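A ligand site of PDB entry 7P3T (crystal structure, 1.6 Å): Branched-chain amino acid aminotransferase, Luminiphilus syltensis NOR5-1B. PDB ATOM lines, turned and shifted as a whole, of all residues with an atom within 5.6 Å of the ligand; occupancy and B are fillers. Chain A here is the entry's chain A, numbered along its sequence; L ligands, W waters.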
ATOM      1  N   PHE A  35     -25.136  -1.501 -17.289  1.00  0.00           N
ATOM      2  CA  PHE A  35     -23.836  -2.143 -17.363  1.00  0.00           C
ATOM      3  C   PHE A  35     -23.777  -3.349 -16.448  1.00  0.00           C
ATOM      4  O   PHE A  35     -24.644  -3.549 -15.594  1.00  0.00           O
ATOM      5  CB  PHE A  35     -22.704  -1.160 -17.037  1.00  0.00           C
ATOM      6  CG  PHE A  35     -22.516  -0.881 -15.552  1.00  0.00           C
ATOM      7  CD1 PHE A  35     -23.294   0.040 -14.880  1.00  0.00           C
ATOM      8  CD2 PHE A  35     -21.544  -1.555 -14.823  1.00  0.00           C
ATOM      9  CE1 PHE A  35     -23.094   0.302 -13.556  1.00  0.00           C
ATOM     10  CE2 PHE A  35     -21.353  -1.297 -13.489  1.00  0.00           C
ATOM     11  CZ  PHE A  35     -22.126  -0.371 -12.849  1.00  0.00           C
ATOM     12  N   ASP A  36     -22.740  -4.161 -16.628  1.00  0.00           N
ATOM     13  CA  ASP A  36     -22.420  -5.206 -15.689  1.00  0.00           C
ATOM     14  C   ASP A  36     -20.908  -5.341 -15.627  1.00  0.00           C
ATOM     15  O   ASP A  36     -20.182  -4.742 -16.441  1.00  0.00           O
ATOM     16  CB  ASP A  36     -23.113  -6.519 -16.060  1.00  0.00           C
ATOM     17  CG  ASP A  36     -23.569  -7.275 -14.831  1.00  0.00           C
ATOM     18  OD1 ASP A  36     -22.704  -7.711 -14.051  1.00  0.00           O
ATOM     19  OD2 ASP A  36     -24.804  -7.400 -14.635  1.00  0.00           O
ATOM     20  N   VAL A  37     -20.443  -6.070 -14.622  1.00  0.00           N
ATOM     21  CA  VAL A  37     -19.019  -6.266 -14.387  1.00  0.00           C
ATOM     22  C   VAL A  37     -18.782  -7.710 -13.996  1.00  0.00           C
ATOM     23  O   VAL A  37     -19.345  -8.201 -13.010  1.00  0.00           O
ATOM     24  CB  VAL A  37     -18.481  -5.361 -13.265  1.00  0.00           C
ATOM     25  CG1 VAL A  37     -16.989  -5.624 -13.063  1.00  0.00           C
ATOM     26  CG2 VAL A  37     -18.729  -3.911 -13.586  1.00  0.00           C
ATOM     27  N   HIS A  51     -23.551 -13.310 -15.253  1.00  0.00           N
ATOM     28  CA  HIS A  51     -23.460 -11.866 -15.414  1.00  0.00           C
ATOM     29  C   HIS A  51     -24.141 -11.425 -16.693  1.00  0.00           C
ATOM     30  O   HIS A  51     -24.784 -10.375 -16.724  1.00  0.00           O
ATOM     31  CB  HIS A  51     -21.994 -11.428 -15.371  1.00  0.00           C
ATOM     32  CG  HIS A  51     -21.454 -11.337 -13.975  1.00  0.00           C
ATOM     33  ND1 HIS A  51     -21.590 -10.225 -13.187  1.00  0.00           N
ATOM     34  CD2 HIS A  51     -20.845 -12.275 -13.193  1.00  0.00           C
ATOM     35  CE1 HIS A  51     -21.056 -10.446 -12.007  1.00  0.00           C
ATOM     36  NE2 HIS A  51     -20.585 -11.681 -11.979  1.00  0.00           N
ATOM     37  N   ARG A  54     -27.847 -11.274 -16.064  1.00  0.00           N
ATOM     38  CA  ARG A  54     -28.271 -10.082 -15.344  1.00  0.00           C
ATOM     39  C   ARG A  54     -28.225  -8.857 -16.238  1.00  0.00           C
ATOM     40  O   ARG A  54     -29.144  -8.016 -16.207  1.00  0.00           O
ATOM     41  CB  ARG A  54     -27.386  -9.872 -14.100  1.00  0.00           C
ATOM     42  CG  ARG A  54     -27.915  -8.798 -13.203  1.00  0.00           C
ATOM     43  CD  ARG A  54     -27.168  -8.745 -11.902  1.00  0.00           C
ATOM     44  NE  ARG A  54     -25.799  -8.313 -12.093  1.00  0.00           N
ATOM     45  CZ  ARG A  54     -24.887  -8.244 -11.130  1.00  0.00           C
ATOM     46  NH1 ARG A  54     -25.196  -8.619  -9.917  1.00  0.00           N
ATOM     47  NH2 ARG A  54     -23.650  -7.837 -11.398  1.00  0.00           N
ATOM     48  N   LYS A 154     -28.511  -2.276 -12.645  1.00  0.00           N
ATOM     49  CA  LYS A 154     -27.104  -1.923 -12.607  1.00  0.00           C
ATOM     50  C   LYS A 154     -26.932  -0.952 -13.764  1.00  0.00           C
ATOM     51  O   LYS A 154     -26.941  -1.356 -14.932  1.00  0.00           O
ATOM     52  CB  LYS A 154     -26.205  -3.137 -12.741  1.00  0.00           C
ATOM     53  CG  LYS A 154     -24.854  -2.951 -12.061  1.00  0.00           C
ATOM     54  CD  LYS A 154     -24.084  -4.258 -11.914  1.00  0.00           C
ATOM     55  CE  LYS A 154     -22.763  -4.035 -11.218  1.00  0.00           C
ATOM     56  NZ  LYS A 154     -22.918  -3.684  -9.764  1.00  0.00           N
ATOM     57  N   ARG A 158     -25.367   6.987 -11.059  1.00  0.00           N
ATOM     58  CA  ARG A 158     -24.743   6.737  -9.771  1.00  0.00           C
ATOM     59  C   ARG A 158     -24.193   8.004  -9.113  1.00  0.00           C
ATOM     60  O   ARG A 158     -23.381   7.908  -8.190  1.00  0.00           O
ATOM     61  CB  ARG A 158     -23.672   5.645  -9.915  1.00  0.00           C
ATOM     62  CG  ARG A 158     -24.257   4.290 -10.215  1.00  0.00           C
ATOM     63  CD  ARG A 158     -23.305   3.243 -10.760  1.00  0.00           C
ATOM     64  NE  ARG A 158     -22.488   2.599  -9.737  1.00  0.00           N
ATOM     65  CZ  ARG A 158     -22.799   1.449  -9.127  1.00  0.00           C
ATOM     66  NH1 ARG A 158     -21.980   0.959  -8.213  1.00  0.00           N
ATOM     67  NH2 ARG A 158     -23.908   0.779  -9.437  1.00  0.00           N
ATOM     68  N   TRP A 178     -26.263   2.107   2.765  1.00  0.00           N
ATOM     69  CA  TRP A 178     -27.485   2.878   2.875  1.00  0.00           C
ATOM     70  C   TRP A 178     -28.656   1.996   3.283  1.00  0.00           C
ATOM     71  O   TRP A 178     -28.637   0.771   3.133  1.00  0.00           O
ATOM     72  CB  TRP A 178     -27.815   3.630   1.579  1.00  0.00           C
ATOM     73  CG  TRP A 178     -27.979   2.847   0.352  1.00  0.00           C
ATOM     74  CD1 TRP A 178     -29.044   2.077   0.015  1.00  0.00           C
ATOM     75  CD2 TRP A 178     -27.065   2.791  -0.767  1.00  0.00           C
ATOM     76  NE1 TRP A 178     -28.857   1.543  -1.242  1.00  0.00           N
ATOM     77  CE2 TRP A 178     -27.652   1.975  -1.743  1.00  0.00           C
ATOM     78  CE3 TRP A 178     -25.824   3.364  -1.020  1.00  0.00           C
ATOM     79  CZ2 TRP A 178     -27.032   1.696  -2.957  1.00  0.00           C
ATOM     80  CZ3 TRP A 178     -25.213   3.098  -2.217  1.00  0.00           C
ATOM     81  CH2 TRP A 178     -25.812   2.268  -3.170  1.00  0.00           C
ATOM     82  N   GLU A 187     -27.506  -2.026   1.099  1.00  0.00           N
ATOM     83  CA  GLU A 187     -26.260  -2.386   0.417  1.00  0.00           C
ATOM     84  C   GLU A 187     -25.359  -1.161   0.383  1.00  0.00           C
ATOM     85  O   GLU A 187     -25.711  -0.092   0.897  1.00  0.00           O
ATOM     86  CB  GLU A 187     -26.557  -2.913  -0.990  1.00  0.00           C
ATOM     87  CG  GLU A 187     -27.246  -1.862  -1.861  1.00  0.00           C
ATOM     88  CD  GLU A 187     -27.601  -2.352  -3.257  1.00  0.00           C
ATOM     89  OE1 GLU A 187     -27.077  -3.394  -3.680  1.00  0.00           O
ATOM     90  OE2 GLU A 187     -28.395  -1.663  -3.932  1.00  0.00           O
ATOM     91  N   SER A 188     -24.204  -1.303  -0.262  1.00  0.00           N
ATOM     92  CA  SER A 188     -23.346  -0.190  -0.628  1.00  0.00           C
ATOM     93  C   SER A 188     -23.299  -0.070  -2.143  1.00  0.00           C
ATOM     94  O   SER A 188     -23.870  -0.891  -2.873  1.00  0.00           O
ATOM     95  CB  SER A 188     -21.950  -0.360  -0.047  1.00  0.00           C
ATOM     96  OG  SER A 188     -21.267  -1.404  -0.739  1.00  0.00           O
ATOM     97  N   ALA A 189     -22.589   0.954  -2.633  1.00  0.00           N
ATOM     98  CA  ALA A 189     -22.549   1.184  -4.076  1.00  0.00           C
ATOM     99  C   ALA A 189     -21.926   0.018  -4.826  1.00  0.00           C
ATOM    100  O   ALA A 189     -22.301  -0.280  -5.966  1.00  0.00           O
ATOM    101  CB  ALA A 189     -21.757   2.456  -4.394  1.00  0.00           C
ATOM    102  N   ALA A 190     -20.950  -0.643  -4.206  1.00  0.00           N
ATOM    103  CA  ALA A 190     -20.182  -1.686  -4.843  1.00  0.00           C
ATOM    104  C   ALA A 190     -20.521  -3.079  -4.345  1.00  0.00           C
ATOM    105  O   ALA A 190     -20.113  -4.044  -4.998  1.00  0.00           O
ATOM    106  CB  ALA A 190     -18.678  -1.442  -4.642  1.00  0.00           C
ATOM    107  N   SER A 191     -21.233  -3.212  -3.235  1.00  0.00           N
ATOM    108  CA  SER A 191     -21.250  -4.477  -2.525  1.00  0.00           C
ATOM    109  C   SER A 191     -22.616  -4.757  -1.924  1.00  0.00           C
ATOM    110  O   SER A 191     -23.407  -3.852  -1.651  1.00  0.00           O
ATOM    111  CB  SER A 191     -20.238  -4.487  -1.364  1.00  0.00           C
ATOM    112  OG  SER A 191     -18.929  -4.133  -1.774  1.00  0.00           O
ATOM    113  N   ASN A 192     -22.865  -6.037  -1.678  1.00  0.00           N
ATOM    114  CA  ASN A 192     -23.949  -6.461  -0.823  1.00  0.00           C
ATOM    115  C   ASN A 192     -23.417  -6.729   0.582  1.00  0.00           C
ATOM    116  O   ASN A 192     -22.228  -6.852   0.823  1.00  0.00           O
ATOM    117  CB  ASN A 192     -24.633  -7.702  -1.404  1.00  0.00           C
ATOM    118  CG  ASN A 192     -25.351  -7.392  -2.714  1.00  0.00           C
ATOM    119  OD1 ASN A 192     -24.949  -7.861  -3.778  1.00  0.00           O
ATOM    120  ND2 ASN A 192     -26.393  -6.587  -2.638  1.00  0.00           N
ATOM    121  N   LEU A 209     -29.484  -4.326  -5.439  1.00  0.00           N
ATOM    122  CA  LEU A 209     -28.986  -5.070  -6.587  1.00  0.00           C
ATOM    123  C   LEU A 209     -28.697  -6.487  -6.112  1.00  0.00           C
ATOM    124  O   LEU A 209     -28.051  -6.702  -5.084  1.00  0.00           O
ATOM    125  CB  LEU A 209     -27.717  -4.407  -7.115  1.00  0.00           C
ATOM    126  CG  LEU A 209     -27.068  -4.869  -8.417  1.00  0.00           C
ATOM    127  CD1 LEU A 209     -26.277  -6.127  -8.165  1.00  0.00           C
ATOM    128  CD2 LEU A 209     -28.092  -5.037  -9.506  1.00  0.00           C
ATOM    129  N   ARG A 210     -29.228  -7.477  -6.827  1.00  0.00           N
ATOM    130  CA  ARG A 210     -29.007  -8.889  -6.459  1.00  0.00           C
ATOM    131  C   ARG A 210     -27.649  -9.317  -7.009  1.00  0.00           C
ATOM    132  O   ARG A 210     -27.562  -9.764  -8.118  1.00  0.00           O
ATOM    133  CB  ARG A 210     -30.192  -9.749  -6.914  1.00  0.00           C
ATOM    134  CG  ARG A 210     -31.492  -9.402  -6.215  1.00  0.00           C
ATOM    135  CD  ARG A 210     -32.684 -10.260  -6.587  1.00  0.00           C
ATOM    136  NE  ARG A 210     -32.496 -11.625  -6.143  1.00  0.00           N
ATOM    137  CZ  ARG A 210     -32.799 -12.037  -4.929  1.00  0.00           C
ATOM    138  NH1 ARG A 210     -32.572 -13.272  -4.560  1.00  0.00           N
ATOM    139  NH2 ARG A 210     -33.345 -11.194  -4.072  1.00  0.00           N
ATOM    140  N   GLY A 211     -26.633  -9.170  -6.179  1.00  0.00           N
ATOM    141  CA  GLY A 211     -25.269  -9.419  -6.591  1.00  0.00           C
ATOM    142  C   GLY A 211     -25.047 -10.875  -6.980  1.00  0.00           C
ATOM    143  O   GLY A 211     -25.666 -11.784  -6.447  1.00  0.00           O
ATOM    144  N   ILE A 212     -24.126 -11.070  -7.908  1.00  0.00           N
ATOM    145  CA  ILE A 212     -23.719 -12.430  -8.265  1.00  0.00           C
ATOM    146  C   ILE A 212     -22.818 -13.010  -7.174  1.00  0.00           C
ATOM    147  O   ILE A 212     -22.846 -14.222  -6.903  1.00  0.00           O
ATOM    148  CB  ILE A 212     -23.020 -12.435  -9.631  1.00  0.00           C
ATOM    149  CG1 ILE A 212     -23.915 -11.946 -10.779  1.00  0.00           C
ATOM    150  CG2 ILE A 212     -22.514 -13.832  -9.983  1.00  0.00           C
ATOM    151  CD1 ILE A 212     -25.289 -12.551 -10.811  1.00  0.00           C
ATOM    152  N   THR A 213     -21.972 -12.172  -6.586  1.00  0.00           N
ATOM    153  CA  THR A 213     -21.190 -12.638  -5.441  1.00  0.00           C
ATOM    154  C   THR A 213     -22.126 -13.047  -4.305  1.00  0.00           C
ATOM    155  O   THR A 213     -21.971 -14.109  -3.713  1.00  0.00           O
ATOM    156  CB  THR A 213     -20.208 -11.554  -4.958  1.00  0.00           C
ATOM    157  OG1 THR A 213     -19.501 -10.967  -6.056  1.00  0.00           O
ATOM    158  CG2 THR A 213     -19.198 -12.172  -4.019  1.00  0.00           C
ATOM    159  N   ARG A 214     -23.147 -12.230  -4.050  1.00  0.00           N
ATOM    160  CA  ARG A 214     -24.168 -12.590  -3.078  1.00  0.00           C
ATOM    161  C   ARG A 214     -24.792 -13.944  -3.363  1.00  0.00           C
ATOM    162  O   ARG A 214     -24.939 -14.789  -2.460  1.00  0.00           O
ATOM    163  CB  ARG A 214     -25.230 -11.479  -3.075  1.00  0.00           C
ATOM    164  CG  ARG A 214     -26.432 -11.685  -2.187  1.00  0.00           C
ATOM    165  CD  ARG A 214     -27.435 -10.571  -2.493  1.00  0.00           C
ATOM    166  NE  ARG A 214     -28.636 -10.599  -1.657  1.00  0.00           N
ATOM    167  CZ  ARG A 214     -29.704 -11.353  -1.883  1.00  0.00           C
ATOM    168  NH1 ARG A 214     -29.747 -12.208  -2.911  1.00  0.00           N
ATOM    169  NH2 ARG A 214     -30.745 -11.289  -1.039  1.00  0.00           N
ATOM    170  N   CYS A 247     -19.631  -8.043   0.142  1.00  0.00           N
ATOM    171  CA  CYS A 247     -19.157  -8.862  -0.966  1.00  0.00           C
ATOM    172  C   CYS A 247     -19.420  -8.157  -2.280  1.00  0.00           C
ATOM    173  O   CYS A 247     -20.413  -7.437  -2.436  1.00  0.00           O
ATOM    174  CB  CYS A 247     -19.793 -10.260  -0.966  1.00  0.00           C
ATOM    175  SG  CYS A 247     -21.576 -10.335  -1.176  1.00  0.00           S
ATOM    176  N   SER A 248     -18.528  -8.414  -3.227  1.00  0.00           N
ATOM    177  CA  SER A 248     -18.515  -7.767  -4.534  1.00  0.00           C
ATOM    178  C   SER A 248     -17.669  -8.572  -5.504  1.00  0.00           C
ATOM    179  O   SER A 248     -16.713  -9.252  -5.113  1.00  0.00           O
ATOM    180  CB  SER A 248     -17.984  -6.340  -4.411  1.00  0.00           C
ATOM    181  OG  SER A 248     -17.916  -5.676  -5.663  1.00  0.00           O
ATOM    182  N   THR A 249     -17.997  -8.465  -6.788  1.00  0.00           N
ATOM    183  CA  THR A 249     -17.067  -8.943  -7.800  1.00  0.00           C
ATOM    184  C   THR A 249     -15.699  -8.298  -7.633  1.00  0.00           C
ATOM    185  O   THR A 249     -14.669  -8.906  -7.980  1.00  0.00           O
ATOM    186  CB  THR A 249     -17.630  -8.698  -9.193  1.00  0.00           C
ATOM    187  OG1 THR A 249     -18.822  -9.471  -9.369  1.00  0.00           O
ATOM    188  CG2 THR A 249     -16.637  -9.143 -10.226  1.00  0.00           C
ATOM    189  N   ALA A 250     -15.650  -7.065  -7.116  1.00  0.00           N
ATOM    190  CA  ALA A 250     -14.388  -6.400  -6.781  1.00  0.00           C
ATOM    191  C   ALA A 250     -13.938  -6.917  -5.420  1.00  0.00           C
ATOM    192  O   ALA A 250     -14.252  -6.338  -4.385  1.00  0.00           O
ATOM    193  CB  ALA A 250     -14.540  -4.900  -6.764  1.00  0.00           C
HETATM  194  N1  LIG L   1     -24.465  -3.511  -5.014  1.00  0.00           N
HETATM  195  C1  LIG L   1     -24.565  -2.626  -6.061  1.00  0.00           C
HETATM  196  C2  LIG L   1     -25.395  -1.394  -5.869  1.00  0.00           C
HETATM  197  C3  LIG L   1     -23.915  -2.863  -7.272  1.00  0.00           C
HETATM  198  O1  LIG L   1     -24.050  -1.963  -8.277  1.00  0.00           O
HETATM  199  C4  LIG L   1     -23.150  -4.043  -7.406  1.00  0.00           C
HETATM  200  C5  LIG L   1     -22.793  -4.559  -8.779  1.00  0.00           C
HETATM  201  C6  LIG L   1     -23.049  -4.910  -6.321  1.00  0.00           C
HETATM  202  C7  LIG L   1     -23.723  -4.664  -5.138  1.00  0.00           C
HETATM  203  C8  LIG L   1     -22.206  -6.174  -6.386  1.00  0.00           C
HETATM  204  O2  LIG L   1     -22.746  -7.096  -7.282  1.00  0.00           O
HETATM  205  P1  LIG L   1     -21.788  -8.318  -7.816  1.00  0.00           P
HETATM  206  O3  LIG L   1     -22.587  -9.006  -8.873  1.00  0.00           O
HETATM  207  O4  LIG L   1     -20.521  -7.669  -8.340  1.00  0.00           O
HETATM  208  O5  LIG L   1     -21.484  -9.275  -6.674  1.00  0.00           O
HETATM  209  O   HOH W   1     -22.744  -9.395  -4.333  1.00  0.00           O
HETATM  210  O   HOH W   2     -28.759  -0.947  -6.541  1.00  0.00           O
HETATM  211  O   HOH W   3     -27.106  -0.905  -8.934  1.00  0.00           O
HETATM  212  O   HOH W   4     -20.571  -6.805 -10.903  1.00  0.00           O
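The backbone NH of Thr 249 lies within hydrogen-bond range of the side-chain hydroxyl of Thr 213, at 3.0 Å. OG1 of Thr 213 lies close to O of Ser 248 (3.4 Å). The guanidinium group of Arg 54 lies within hydrogen-bond range of the backbone carbonyl oxygen of Arg 210. OE1 of Glu 187 sits at hydrogen-bond distance from N of Leu 209 (3.1 Å). The guanidinium group (NH1) of Arg 158 sits at hydrogen-bond distance from the backbone carbonyl oxygen (O) of Ala 189 (2.6 Å). OG of Ser 188 is in hydrogen-bond range of N of Ser 191. The backbone carbonyl oxygen (O) of Leu 209 lies within hydrogen-bond range of the side-chain amide nitrogen (ND2) of Asn 192, 3.0 Å away. ND1 of His 51 sits at hydrogen-bond distance from OD1 of Asp 36, 2.9 Å away.
The side-chain carboxylate (OE1) of Glu 187 sits close to a nitrogen (N1) of the ligand (2.9 Å). The backbone carbonyl oxygen of Ser 188 sits close to a nitrogen (N1) of the ligand, at 3.4 Å. Residues that only touch the ligand: His 51, Ala 190, Ser 191, Asn 192, Leu 209, Gly 211 and Ser 248. Hydrophobic or aromatic side chains that line the ligand: His 51, Leu 209 and Ile 212.
Water W1 lies within hydrogen-bond range of O5 of the ligand (2.7 Å), OD1 of Asn 192 (2.7 Å), N of Arg 214 (2.9 Å) and SG of Cys 247 (3.5 Å). Water W4 lies within hydrogen-bond range of an oxygen (O4) of the ligand (2.7 Å), the backbone carbonyl oxygen (O) of Val 37 (2.8 Å) and the guanidinium group (NH2) of Arg 54 (3.3 Å).
The side-chain amino group (NZ) of Lys 154 is bonded to a carbon (C5) of the ligand (1.3 Å). An oxygen (O5) of the ligand is in hydrogen-bond range of the backbone NH (N) of Thr 213 (2.9 Å). The side-chain hydroxyl of Thr 213 is in hydrogen-bond range of an oxygen (O5) of the ligand, at 2.7 Å. The backbone NH (N) of Thr 249 is in hydrogen-bond range of an oxygen (O4) of the ligand (3.1 Å). The side-chain hydroxyl (OG1) of Thr 249 sits at hydrogen-bond distance from an oxygen (O4) of the ligand (2.7 Å). O3 of the ligand is in hydrogen-bond range of N of Ile 212 (2.7 Å). The guanidinium group (NH1) of Arg 54 is in salt-bridge range of an oxygen (O3) of the ligand (2.8 Å). An oxygen (O1) of the ligand is in hydrogen-bond range of the guanidinium group of Arg 158, 3.0 Å away. O of Ala 189 lies close to O1 of the ligand (3.4 Å).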
